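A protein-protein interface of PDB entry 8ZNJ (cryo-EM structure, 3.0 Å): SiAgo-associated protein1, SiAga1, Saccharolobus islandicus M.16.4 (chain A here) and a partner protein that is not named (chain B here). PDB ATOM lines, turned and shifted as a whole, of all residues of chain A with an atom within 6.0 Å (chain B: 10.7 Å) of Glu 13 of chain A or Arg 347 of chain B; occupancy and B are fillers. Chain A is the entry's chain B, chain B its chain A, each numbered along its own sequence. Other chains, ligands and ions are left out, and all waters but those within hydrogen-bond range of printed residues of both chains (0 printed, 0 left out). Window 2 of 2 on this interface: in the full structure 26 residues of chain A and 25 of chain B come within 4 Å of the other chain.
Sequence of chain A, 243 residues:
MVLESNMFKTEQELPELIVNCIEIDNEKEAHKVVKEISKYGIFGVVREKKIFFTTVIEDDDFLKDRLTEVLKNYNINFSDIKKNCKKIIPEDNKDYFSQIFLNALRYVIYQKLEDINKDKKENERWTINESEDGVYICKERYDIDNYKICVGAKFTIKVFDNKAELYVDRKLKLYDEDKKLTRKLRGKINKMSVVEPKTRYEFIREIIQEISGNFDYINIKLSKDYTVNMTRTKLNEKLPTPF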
ATOM      1  N   THR A  10       1.857  14.648  21.651  1.00  0.00           N
ATOM      2  CA  THR A  10       3.250  15.034  21.510  1.00  0.00           C
ATOM      3  C   THR A  10       3.677  15.858  22.724  1.00  0.00           C
ATOM      4  O   THR A  10       2.878  16.174  23.609  1.00  0.00           O
ATOM      5  CB  THR A  10       3.469  15.822  20.219  1.00  0.00           C
ATOM      6  OG1 THR A  10       2.414  16.773  20.047  1.00  0.00           O
ATOM      7  CG2 THR A  10       3.507  14.886  19.027  1.00  0.00           C
ATOM      8  N   GLU A  11       4.959  16.209  22.760  1.00  0.00           N
ATOM      9  CA  GLU A  11       5.526  16.966  23.869  1.00  0.00           C
ATOM     10  C   GLU A  11       5.995  18.351  23.459  1.00  0.00           C
ATOM     11  O   GLU A  11       5.894  19.288  24.252  1.00  0.00           O
ATOM     12  CB  GLU A  11       6.702  16.213  24.520  1.00  0.00           C
ATOM     13  CG  GLU A  11       7.758  15.597  23.584  1.00  0.00           C
ATOM     14  CD  GLU A  11       7.243  14.472  22.694  1.00  0.00           C
ATOM     15  OE1 GLU A  11       8.010  14.029  21.813  1.00  0.00           O
ATOM     16  OE2 GLU A  11       6.111  13.993  22.903  1.00  0.00           O
ATOM     17  N   GLN A  12       6.508  18.501  22.245  1.00  0.00           N
ATOM     18  CA  GLN A  12       6.859  19.791  21.676  1.00  0.00           C
ATOM     19  C   GLN A  12       5.938  20.082  20.496  1.00  0.00           C
ATOM     20  O   GLN A  12       5.106  19.259  20.105  1.00  0.00           O
ATOM     21  CB  GLN A  12       8.329  19.810  21.250  1.00  0.00           C
ATOM     22  CG  GLN A  12       9.280  20.323  22.317  1.00  0.00           C
ATOM     23  CD  GLN A  12       9.678  19.248  23.309  1.00  0.00           C
ATOM     24  OE1 GLN A  12       8.836  18.501  23.803  1.00  0.00           O
ATOM     25  NE2 GLN A  12      10.970  19.165  23.602  1.00  0.00           N
ATOM     26  N   GLU A  13       6.091  21.271  19.924  1.00  0.00           N
ATOM     27  CA  GLU A  13       5.325  21.625  18.740  1.00  0.00           C
ATOM     28  C   GLU A  13       5.807  20.801  17.553  1.00  0.00           C
ATOM     29  O   GLU A  13       7.011  20.719  17.291  1.00  0.00           O
ATOM     30  CB  GLU A  13       5.464  23.115  18.440  1.00  0.00           C
ATOM     31  CG  GLU A  13       5.105  24.028  19.601  1.00  0.00           C
ATOM     32  CD  GLU A  13       5.490  25.471  19.342  1.00  0.00           C
ATOM     33  OE1 GLU A  13       5.357  25.925  18.187  1.00  0.00           O
ATOM     34  OE2 GLU A  13       5.931  26.149  20.293  1.00  0.00           O
ATOM     35  N   LEU A  14       4.867  20.185  16.841  1.00  0.00           N
ATOM     36  CA  LEU A  14       5.179  19.387  15.664  1.00  0.00           C
ATOM     37  C   LEU A  14       6.120  20.162  14.748  1.00  0.00           C
ATOM     38  O   LEU A  14       5.707  21.159  14.143  1.00  0.00           O
ATOM     39  CB  LEU A  14       3.901  19.023  14.914  1.00  0.00           C
ATOM     40  CG  LEU A  14       2.961  18.037  15.602  1.00  0.00           C
ATOM     41  CD1 LEU A  14       1.575  18.117  14.981  1.00  0.00           C
ATOM     42  CD2 LEU A  14       3.518  16.627  15.518  1.00  0.00           C
ATOM     43  N   PRO A  15       7.378  19.744  14.609  1.00  0.00           N
ATOM     44  CA  PRO A  15       8.314  20.516  13.786  1.00  0.00           C
ATOM     45  C   PRO A  15       7.847  20.616  12.342  1.00  0.00           C
ATOM     46  O   PRO A  15       7.114  19.768  11.833  1.00  0.00           O
ATOM     47  CB  PRO A  15       9.623  19.725  13.897  1.00  0.00           C
ATOM     48  CG  PRO A  15       9.503  18.966  15.162  1.00  0.00           C
ATOM     49  CD  PRO A  15       8.050  18.635  15.308  1.00  0.00           C
ATOM     50  N   GLU A  16       8.275  21.695  11.692  1.00  0.00           N
ATOM     51  CA  GLU A  16       7.945  21.975  10.302  1.00  0.00           C
ATOM     52  C   GLU A  16       8.021  20.715   9.449  1.00  0.00           C
ATOM     53  O   GLU A  16       9.050  20.032   9.420  1.00  0.00           O
ATOM     54  CB  GLU A  16       8.911  23.037   9.763  1.00  0.00           C
ATOM     55  CG  GLU A  16       8.742  23.414   8.295  1.00  0.00           C
ATOM     56  CD  GLU A  16       7.337  23.858   7.939  1.00  0.00           C
ATOM     57  OE1 GLU A  16       6.380  23.109   8.213  1.00  0.00           O
ATOM     58  OE2 GLU A  16       7.191  24.965   7.380  1.00  0.00           O
ATOM     59  N   ILE A  89       3.146  23.545   8.013  1.00  0.00           N
ATOM     60  CA  ILE A  89       2.945  23.640   9.453  1.00  0.00           C
ATOM     61  C   ILE A  89       1.621  22.950   9.770  1.00  0.00           C
ATOM     62  O   ILE A  89       0.589  23.333   9.195  1.00  0.00           O
ATOM     63  CB  ILE A  89       2.928  25.098   9.928  1.00  0.00           C
ATOM     64  CG1 ILE A  89       4.337  25.692   9.872  1.00  0.00           C
ATOM     65  CG2 ILE A  89       2.366  25.191  11.341  1.00  0.00           C
ATOM     66  CD1 ILE A  89       5.188  25.382  11.086  1.00  0.00           C
ATOM     67  N   GLU A  91      -0.603  23.121  12.046  1.00  0.00           N
ATOM     68  CA  GLU A  91      -1.706  23.963  12.498  1.00  0.00           C
ATOM     69  C   GLU A  91      -2.376  24.675  11.328  1.00  0.00           C
ATOM     70  O   GLU A  91      -3.609  24.721  11.244  1.00  0.00           O
ATOM     71  CB  GLU A  91      -1.204  24.979  13.522  1.00  0.00           C
ATOM     72  CG  GLU A  91      -1.781  24.785  14.911  1.00  0.00           C
ATOM     73  CD  GLU A  91      -3.268  25.060  14.970  1.00  0.00           C
ATOM     74  OE1 GLU A  91      -3.894  25.184  13.896  1.00  0.00           O
ATOM     75  OE2 GLU A  91      -3.814  25.154  16.088  1.00  0.00           O
ATOM     76  N   ASP A 161      -2.957  23.324  19.177  1.00  0.00           N
ATOM     77  CA  ASP A 161      -1.813  24.149  19.554  1.00  0.00           C
ATOM     78  C   ASP A 161      -0.542  23.652  18.871  1.00  0.00           C
ATOM     79  O   ASP A 161       0.541  23.634  19.458  1.00  0.00           O
ATOM     80  CB  ASP A 161      -1.638  24.181  21.072  1.00  0.00           C
ATOM     81  CG  ASP A 161      -0.773  25.337  21.536  1.00  0.00           C
ATOM     82  OD1 ASP A 161      -0.697  26.355  20.815  1.00  0.00           O
ATOM     83  OD2 ASP A 161      -0.167  25.229  22.622  1.00  0.00           O
ATOM     84  N   ASN A 162      -0.680  23.244  17.611  1.00  0.00           N
ATOM     85  CA  ASN A 162       0.442  22.717  16.837  1.00  0.00           C
ATOM     86  C   ASN A 162       1.081  21.521  17.536  1.00  0.00           C
ATOM     87  O   ASN A 162       2.303  21.374  17.561  1.00  0.00           O
ATOM     88  CB  ASN A 162       1.481  23.806  16.571  1.00  0.00           C
ATOM     89  CG  ASN A 162       2.154  23.652  15.223  1.00  0.00           C
ATOM     90  OD1 ASN A 162       1.505  23.353  14.221  1.00  0.00           O
ATOM     91  ND2 ASN A 162       3.465  23.857  15.191  1.00  0.00           N
ATOM     92  N   LYS A 163       0.247  20.666  18.125  1.00  0.00           N
ATOM     93  CA  LYS A 163       0.705  19.430  18.742  1.00  0.00           C
ATOM     94  C   LYS A 163      -0.247  18.309  18.355  1.00  0.00           C
ATOM     95  O   LYS A 163      -1.464  18.504  18.322  1.00  0.00           O
ATOM     96  CB  LYS A 163       0.782  19.553  20.268  1.00  0.00           C
ATOM     97  CG  LYS A 163       1.699  20.662  20.752  1.00  0.00           C
ATOM     98  CD  LYS A 163       1.411  21.036  22.196  1.00  0.00           C
ATOM     99  CE  LYS A 163       1.749  19.905  23.158  1.00  0.00           C
ATOM    100  NZ  LYS A 163       3.044  19.238  22.847  1.00  0.00           N
ATOM    101  N   SER B   2       0.379  24.765  30.454  1.00  0.00           N
ATOM    102  CA  SER B   2       0.490  23.444  29.849  1.00  0.00           C
ATOM    103  C   SER B   2      -0.817  22.677  30.011  1.00  0.00           C
ATOM    104  O   SER B   2      -1.881  23.283  30.175  1.00  0.00           O
ATOM    105  CB  SER B   2       1.650  22.666  30.475  1.00  0.00           C
ATOM    106  OG  SER B   2       2.072  21.607  29.633  1.00  0.00           O
ATOM    107  N   LYS B 299     -18.008  33.896  13.242  1.00  0.00           N
ATOM    108  CA  LYS B 299     -16.845  34.646  13.697  1.00  0.00           C
ATOM    109  C   LYS B 299     -16.923  36.095  13.234  1.00  0.00           C
ATOM    110  O   LYS B 299     -16.696  37.026  14.016  1.00  0.00           O
ATOM    111  CB  LYS B 299     -15.567  33.982  13.186  1.00  0.00           C
ATOM    112  CG  LYS B 299     -14.288  34.610  13.711  1.00  0.00           C
ATOM    113  CD  LYS B 299     -13.065  33.929  13.127  1.00  0.00           C
ATOM    114  CE  LYS B 299     -11.795  34.697  13.440  1.00  0.00           C
ATOM    115  NZ  LYS B 299     -10.651  34.201  12.628  1.00  0.00           N
ATOM    116  N   LYS B 343      -6.283  22.258  28.906  1.00  0.00           N
ATOM    117  CA  LYS B 343      -5.133  22.485  28.037  1.00  0.00           C
ATOM    118  C   LYS B 343      -5.225  23.907  27.509  1.00  0.00           C
ATOM    119  O   LYS B 343      -6.087  24.204  26.676  1.00  0.00           O
ATOM    120  CB  LYS B 343      -5.104  21.495  26.877  1.00  0.00           C
ATOM    121  CG  LYS B 343      -5.220  20.043  27.272  1.00  0.00           C
ATOM    122  CD  LYS B 343      -5.030  19.144  26.063  1.00  0.00           C
ATOM    123  CE  LYS B 343      -6.178  19.282  25.081  1.00  0.00           C
ATOM    124  NZ  LYS B 343      -6.027  18.360  23.930  1.00  0.00           N
ATOM    125  N   LYS B 344      -4.352  24.786  27.988  1.00  0.00           N
ATOM    126  CA  LYS B 344      -4.298  26.128  27.437  1.00  0.00           C
ATOM    127  C   LYS B 344      -3.646  26.100  26.058  1.00  0.00           C
ATOM    128  O   LYS B 344      -2.964  25.142  25.683  1.00  0.00           O
ATOM    129  CB  LYS B 344      -3.530  27.062  28.370  1.00  0.00           C
ATOM    130  CG  LYS B 344      -4.354  27.579  29.535  1.00  0.00           C
ATOM    131  CD  LYS B 344      -3.754  28.843  30.124  1.00  0.00           C
ATOM    132  CE  LYS B 344      -4.338  30.087  29.477  1.00  0.00           C
ATOM    133  NZ  LYS B 344      -3.693  31.332  29.972  1.00  0.00           N
ATOM    134  N   ARG B 345      -3.869  27.164  25.293  1.00  0.00           N
ATOM    135  CA  ARG B 345      -3.330  27.291  23.943  1.00  0.00           C
ATOM    136  C   ARG B 345      -2.459  28.538  23.888  1.00  0.00           C
ATOM    137  O   ARG B 345      -2.972  29.661  23.915  1.00  0.00           O
ATOM    138  CB  ARG B 345      -4.451  27.355  22.908  1.00  0.00           C
ATOM    139  CG  ARG B 345      -3.968  27.265  21.474  1.00  0.00           C
ATOM    140  CD  ARG B 345      -5.053  26.730  20.564  1.00  0.00           C
ATOM    141  NE  ARG B 345      -4.732  26.911  19.152  1.00  0.00           N
ATOM    142  CZ  ARG B 345      -4.991  28.010  18.457  1.00  0.00           C
ATOM    143  NH1 ARG B 345      -5.575  29.057  19.012  1.00  0.00           N
ATOM    144  NH2 ARG B 345      -4.657  28.057  17.171  1.00  0.00           N
ATOM    145  N   LYS B 346      -1.142  28.337  23.804  1.00  0.00           N
ATOM    146  CA  LYS B 346      -0.222  29.467  23.755  1.00  0.00           C
ATOM    147  C   LYS B 346      -0.468  30.320  22.518  1.00  0.00           C
ATOM    148  O   LYS B 346      -0.365  31.551  22.569  1.00  0.00           O
ATOM    149  CB  LYS B 346       1.222  28.962  23.786  1.00  0.00           C
ATOM    150  CG  LYS B 346       2.155  29.642  22.794  1.00  0.00           C
ATOM    151  CD  LYS B 346       3.579  29.137  22.943  1.00  0.00           C
ATOM    152  CE  LYS B 346       3.819  27.897  22.094  1.00  0.00           C
ATOM    153  NZ  LYS B 346       3.822  28.201  20.636  1.00  0.00           N
ATOM    154  N   ARG B 347      -0.787  29.681  21.393  1.00  0.00           N
ATOM    155  CA  ARG B 347      -1.024  30.373  20.128  1.00  0.00           C
ATOM    156  C   ARG B 347      -2.469  30.877  20.109  1.00  0.00           C
ATOM    157  O   ARG B 347      -3.339  30.370  19.401  1.00  0.00           O
ATOM    158  CB  ARG B 347      -0.732  29.431  18.967  1.00  0.00           C
ATOM    159  CG  ARG B 347      -1.102  29.937  17.579  1.00  0.00           C
ATOM    160  CD  ARG B 347      -1.109  28.798  16.565  1.00  0.00           C
ATOM    161  NE  ARG B 347       0.235  28.437  16.129  1.00  0.00           N
ATOM    162  CZ  ARG B 347       1.033  27.585  16.760  1.00  0.00           C
ATOM    163  NH1 ARG B 347       0.649  26.959  17.861  1.00  0.00           N
ATOM    164  NH2 ARG B 347       2.246  27.350  16.271  1.00  0.00           N
ATOM    165  N   TRP B 348      -2.722  31.900  20.925  1.00  0.00           N
ATOM    166  CA  TRP B 348      -4.072  32.426  21.110  1.00  0.00           C
ATOM    167  C   TRP B 348      -4.069  33.943  20.978  1.00  0.00           C
ATOM    168  O   TRP B 348      -3.527  34.644  21.837  1.00  0.00           O
ATOM    169  CB  TRP B 348      -4.643  32.019  22.465  1.00  0.00           C
ATOM    170  CG  TRP B 348      -5.850  32.818  22.834  1.00  0.00           C
ATOM    171  CD1 TRP B 348      -7.079  32.762  22.248  1.00  0.00           C
ATOM    172  CD2 TRP B 348      -5.944  33.804  23.867  1.00  0.00           C
ATOM    173  NE1 TRP B 348      -7.933  33.647  22.853  1.00  0.00           N
ATOM    174  CE2 TRP B 348      -7.260  34.300  23.851  1.00  0.00           C
ATOM    175  CE3 TRP B 348      -5.043  34.315  24.805  1.00  0.00           C
ATOM    176  CZ2 TRP B 348      -7.697  35.282  24.734  1.00  0.00           C
ATOM    177  CZ3 TRP B 348      -5.478  35.288  25.680  1.00  0.00           C
ATOM    178  CH2 TRP B 348      -6.793  35.761  25.640  1.00  0.00           C
ATOM    179  N   ASN B 349      -4.677  34.438  19.902  1.00  0.00           N
ATOM    180  CA  ASN B 349      -5.127  35.819  19.789  1.00  0.00           C
ATOM    181  C   ASN B 349      -4.043  36.829  20.134  1.00  0.00           C
ATOM    182  O   ASN B 349      -4.089  37.443  21.208  1.00  0.00           O
ATOM    183  CB  ASN B 349      -6.338  36.055  20.692  1.00  0.00           C
ATOM    184  CG  ASN B 349      -6.938  37.433  20.507  1.00  0.00           C
ATOM    185  OD1 ASN B 349      -7.181  37.871  19.384  1.00  0.00           O
ATOM    186  ND2 ASN B 349      -7.171  38.128  21.613  1.00  0.00           N
ATOM    187  N   PRO B 350      -3.058  37.027  19.271  1.00  0.00           N
ATOM    188  CA  PRO B 350      -2.163  38.186  19.378  1.00  0.00           C
ATOM    189  C   PRO B 350      -2.820  39.466  18.857  1.00  0.00           C
ATOM    190  O   PRO B 350      -2.232  40.216  18.076  1.00  0.00           O
ATOM    191  CB  PRO B 350      -0.962  37.767  18.528  1.00  0.00           C
ATOM    192  CG  PRO B 350      -1.542  36.867  17.493  1.00  0.00           C
ATOM    193  CD  PRO B 350      -2.679  36.138  18.157  1.00  0.00           C
ATOM    194  N   ASN B 351      -4.057  39.714  19.295  1.00  0.00           N
ATOM    195  CA  ASN B 351      -4.889  40.784  18.750  1.00  0.00           C
ATOM    196  C   ASN B 351      -5.041  40.644  17.237  1.00  0.00           C
ATOM    197  O   ASN B 351      -5.167  41.637  16.518  1.00  0.00           O
ATOM    198  CB  ASN B 351      -4.327  42.161  19.110  1.00  0.00           C
ATOM    199  CG  ASN B 351      -4.715  42.598  20.507  1.00  0.00           C
ATOM    200  OD1 ASN B 351      -4.562  41.846  21.469  1.00  0.00           O
ATOM    201  ND2 ASN B 351      -5.220  43.821  20.627  1.00  0.00           N
ATOM    202  N   ASN B 352      -5.037  39.406  16.751  1.00  0.00           N
ATOM    203  CA  ASN B 352      -5.054  39.107  15.325  1.00  0.00           C
ATOM    204  C   ASN B 352      -6.383  38.559  14.836  1.00  0.00           C
ATOM    205  O   ASN B 352      -6.855  38.964  13.772  1.00  0.00           O
ATOM    206  CB  ASN B 352      -3.948  38.099  14.992  1.00  0.00           C
ATOM    207  CG  ASN B 352      -4.075  37.535  13.591  1.00  0.00           C
ATOM    208  OD1 ASN B 352      -4.548  38.208  12.677  1.00  0.00           O
ATOM    209  ND2 ASN B 352      -3.651  36.288  13.418  1.00  0.00           N
ATOM    210  N   GLY B 353      -7.002  37.650  15.586  1.00  0.00           N
ATOM    211  CA  GLY B 353      -8.243  37.036  15.159  1.00  0.00           C
ATOM    212  C   GLY B 353      -8.262  35.531  15.334  1.00  0.00           C
ATOM    213  O   GLY B 353      -9.178  34.858  14.851  1.00  0.00           O
ATOM    214  N   ASP B 354      -7.259  34.988  16.018  1.00  0.00           N
ATOM    215  CA  ASP B 354      -7.205  33.567  16.351  1.00  0.00           C
ATOM    216  C   ASP B 354      -7.700  33.434  17.787  1.00  0.00           C
ATOM    217  O   ASP B 354      -6.943  33.640  18.737  1.00  0.00           O
ATOM    218  CB  ASP B 354      -5.793  33.022  16.177  1.00  0.00           C
ATOM    219  CG  ASP B 354      -5.538  31.793  17.016  1.00  0.00           C
ATOM    220  OD1 ASP B 354      -4.901  31.920  18.080  1.00  0.00           O
ATOM    221  OD2 ASP B 354      -5.974  30.697  16.608  1.00  0.00           O
ATOM    222  N   TYR B 355      -8.977  33.092  17.944  1.00  0.00           N
ATOM    223  CA  TYR B 355      -9.661  33.245  19.219  1.00  0.00           C
ATOM    224  C   TYR B 355      -9.671  31.989  20.082  1.00  0.00           C
ATOM    225  O   TYR B 355     -10.075  32.072  21.245  1.00  0.00           O
ATOM    226  CB  TYR B 355     -11.106  33.693  18.978  1.00  0.00           C
ATOM    227  CG  TYR B 355     -11.237  35.134  18.540  1.00  0.00           C
ATOM    228  CD1 TYR B 355     -10.751  36.167  19.328  1.00  0.00           C
ATOM    229  CD2 TYR B 355     -11.851  35.459  17.339  1.00  0.00           C
ATOM    230  CE1 TYR B 355     -10.871  37.483  18.932  1.00  0.00           C
ATOM    231  CE2 TYR B 355     -11.976  36.774  16.935  1.00  0.00           C
ATOM    232  CZ  TYR B 355     -11.485  37.780  17.735  1.00  0.00           C
ATOM    233  OH  TYR B 355     -11.608  39.090  17.335  1.00  0.00           O
ATOM    234  N   LEU B 356      -9.245  30.840  19.566  1.00  0.00           N
ATOM    235  CA  LEU B 356      -9.294  29.607  20.349  1.00  0.00           C
ATOM    236  C   LEU B 356      -8.348  29.730  21.539  1.00  0.00           C
ATOM    237  O   LEU B 356      -7.129  29.801  21.370  1.00  0.00           O
ATOM    238  CB  LEU B 356      -8.935  28.411  19.475  1.00  0.00           C
ATOM    239  CG  LEU B 356      -9.247  27.034  20.065  1.00  0.00           C
ATOM    240  CD1 LEU B 356     -10.730  26.722  19.979  1.00  0.00           C
ATOM    241  CD2 LEU B 356      -8.439  25.967  19.354  1.00  0.00           C
ATOM    242  N   HIS B 357      -8.911  29.753  22.747  1.00  0.00           N
ATOM    243  CA  HIS B 357      -8.160  30.015  23.968  1.00  0.00           C
ATOM    244  C   HIS B 357      -7.634  28.739  24.614  1.00  0.00           C
ATOM    245  O   HIS B 357      -6.432  28.623  24.870  1.00  0.00           O
ATOM    246  CB  HIS B 357      -9.041  30.776  24.963  1.00  0.00           C
ATOM    247  CG  HIS B 357      -8.348  31.125  26.242  1.00  0.00           C
ATOM    248  ND1 HIS B 357      -8.252  30.247  27.298  1.00  0.00           N
ATOM    249  CD2 HIS B 357      -7.721  32.258  26.636  1.00  0.00           C
ATOM    250  CE1 HIS B 357      -7.594  30.823  28.288  1.00  0.00           C
ATOM    251  NE2 HIS B 357      -7.260  32.044  27.912  1.00  0.00           N
ATOM    252  N   SER B 358      -8.512  27.782  24.893  1.00  0.00           N
ATOM    253  CA  SER B 358      -8.110  26.560  25.575  1.00  0.00           C
ATOM    254  C   SER B 358      -9.121  25.466  25.260  1.00  0.00           C
ATOM    255  O   SER B 358     -10.130  25.695  24.590  1.00  0.00           O
ATOM    256  CB  SER B 358      -7.993  26.785  27.084  1.00  0.00           C
ATOM    257  OG  SER B 358      -9.256  27.079  27.651  1.00  0.00           O
ATOM    258  N   GLU B 359      -8.830  24.265  25.751  1.00  0.00           N
ATOM    259  CA  GLU B 359      -9.695  23.107  25.584  1.00  0.00           C
ATOM    260  C   GLU B 359      -9.863  22.434  26.936  1.00  0.00           C
ATOM    261  O   GLU B 359      -8.871  22.114  27.600  1.00  0.00           O
ATOM    262  CB  GLU B 359      -9.108  22.129  24.562  1.00  0.00           C
ATOM    263  CG  GLU B 359      -9.754  20.762  24.567  1.00  0.00           C
ATOM    264  CD  GLU B 359      -9.713  20.100  23.208  1.00  0.00           C
ATOM    265  OE1 GLU B 359      -8.704  19.434  22.901  1.00  0.00           O
ATOM    266  OE2 GLU B 359     -10.690  20.245  22.446  1.00  0.00           O
ATOM    267  N   VAL B 395     -13.087  26.327  23.762  1.00  0.00           N
ATOM    268  CA  VAL B 395     -13.361  27.683  24.218  1.00  0.00           C
ATOM    269  C   VAL B 395     -12.666  28.662  23.287  1.00  0.00           C
ATOM    270  O   VAL B 395     -11.471  28.521  23.010  1.00  0.00           O
ATOM    271  CB  VAL B 395     -12.890  27.881  25.669  1.00  0.00           C
ATOM    272  CG1 VAL B 395     -13.057  29.328  26.094  1.00  0.00           C
ATOM    273  CG2 VAL B 395     -13.643  26.953  26.606  1.00  0.00           C
ATOM    274  N   TYR B 396     -13.413  29.642  22.789  1.00  0.00           N
ATOM    275  CA  TYR B 396     -12.859  30.808  22.121  1.00  0.00           C
ATOM    276  C   TYR B 396     -13.159  32.023  22.985  1.00  0.00           C
ATOM    277  O   TYR B 396     -14.266  32.155  23.510  1.00  0.00           O
ATOM    278  CB  TYR B 396     -13.462  31.008  20.729  1.00  0.00           C
ATOM    279  CG  TYR B 396     -13.515  29.768  19.868  1.00  0.00           C
ATOM    280  CD1 TYR B 396     -14.463  28.782  20.093  1.00  0.00           C
ATOM    281  CD2 TYR B 396     -12.631  29.595  18.816  1.00  0.00           C
ATOM    282  CE1 TYR B 396     -14.521  27.653  19.303  1.00  0.00           C
ATOM    283  CE2 TYR B 396     -12.683  28.470  18.019  1.00  0.00           C
ATOM    284  CZ  TYR B 396     -13.630  27.503  18.268  1.00  0.00           C
ATOM    285  OH  TYR B 396     -13.683  26.379  17.479  1.00  0.00           O
ATOM    286  N   SER B 397     -12.178  32.903  23.148  1.00  0.00           N
ATOM    287  CA  SER B 397     -12.382  34.056  24.008  1.00  0.00           C
ATOM    288  C   SER B 397     -11.576  35.235  23.494  1.00  0.00           C
ATOM    289  O   SER B 397     -10.578  35.077  22.788  1.00  0.00           O
ATOM    290  CB  SER B 397     -12.000  33.741  25.456  1.00  0.00           C
ATOM    291  OG  SER B 397     -12.167  34.878  26.283  1.00  0.00           O
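The backbone carbonyl oxygen (O) of His 357 of chain B is in hydrogen-bond range of the backbone NH (N) of Arg 345 of chain B (3.0 Å). N of Leu 14 of chain A lies within hydrogen-bond range of O of Asn 162 of chain A, 2.9 Å away. NH1 of Arg 345 of chain B lies within salt-bridge range of OD2 of Asp 354 of chain B, 2.9 Å away. N of Glu 91 of chain A sits at hydrogen-bond distance from OD1 of Asn 162 of chain A, 3.0 Å away. O of Leu 356 of chain B sits at hydrogen-bond distance from NH1 of Arg 345 of chain B (2.9 Å). O of Arg 347 of chain B sits close to OD1 of Asp 354 of chain B (2.6 Å).
The side-chain carboxylate (OD2) of Asp 161 of chain A sits at hydrogen-bond distance from the backbone NH (N) of Lys 346 of chain B (3.5 Å). The side-chain carboxylate (OE2) of Glu 91 of chain A is in salt-bridge range of the guanidinium group (NH2) of Arg 345 of chain B (3.2 Å). The side-chain carboxylate of Glu 13 of chain A lies within salt-bridge range of the guanidinium group of Arg 347 of chain B (3.9 Å). The side-chain amino group (NZ) of Lys 346 of chain B is in salt-bridge range of the side-chain carboxylate (OE2) of Glu 13 of chain A (3.0 Å). The side-chain carboxylate of Asp 161 of chain A is in salt-bridge range of the guanidinium group of Arg 347 of chain B (3.3 Å).
Glu 13 of chain A touches two residues of chain B. No residue of chain B comes within 4 Å of Leu 14 of chain A. Asp 161 of chain A touches three residues of chain B. Of the printed residues of chain A, Arg 345 of chain B touches Glu 91 (3.2 Å) and Asp 161 (3.5 Å). Of the printed residues of chain B, Glu 91 of chain A touches Arg 345 (3.2 Å). Of the printed residues of chain A, Lys 346 of chain B touches Glu 13 and Asp 161. Glu 359 of chain B touches none of the printed residues of chain A. Gly 353 of chain B touches none of the printed residues of chain A. The nearest residue of chain B that does not touch Glu 13 of chain A is Arg 345 of chain B (9.4 Å).
Among the printed residues, merely in contact across the chains: Asp 161 of chain A with Arg 345 of chain B (3.5 Å) and Asn 162 of chain A with Arg 347 of chain B (3.5 Å).
Of the 22 printed residues of chain B, 3 touch a printed residue of chain A. Printed residues of chain B that touch a printed residue of chain A: Arg 345, Lys 346 and Arg 347. Among the printed residues, Asp or Glu carboxylates within 4 Å of a Lys or Arg side-chain nitrogen of the other chain: Glu 13 of chain A with Lys 346 of chain B, Glu 13 of chain A with Arg 347 of chain B, Glu 91 of chain A with Arg 345 of chain B and Asp 161 of chain A with Arg 347 of chain B.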
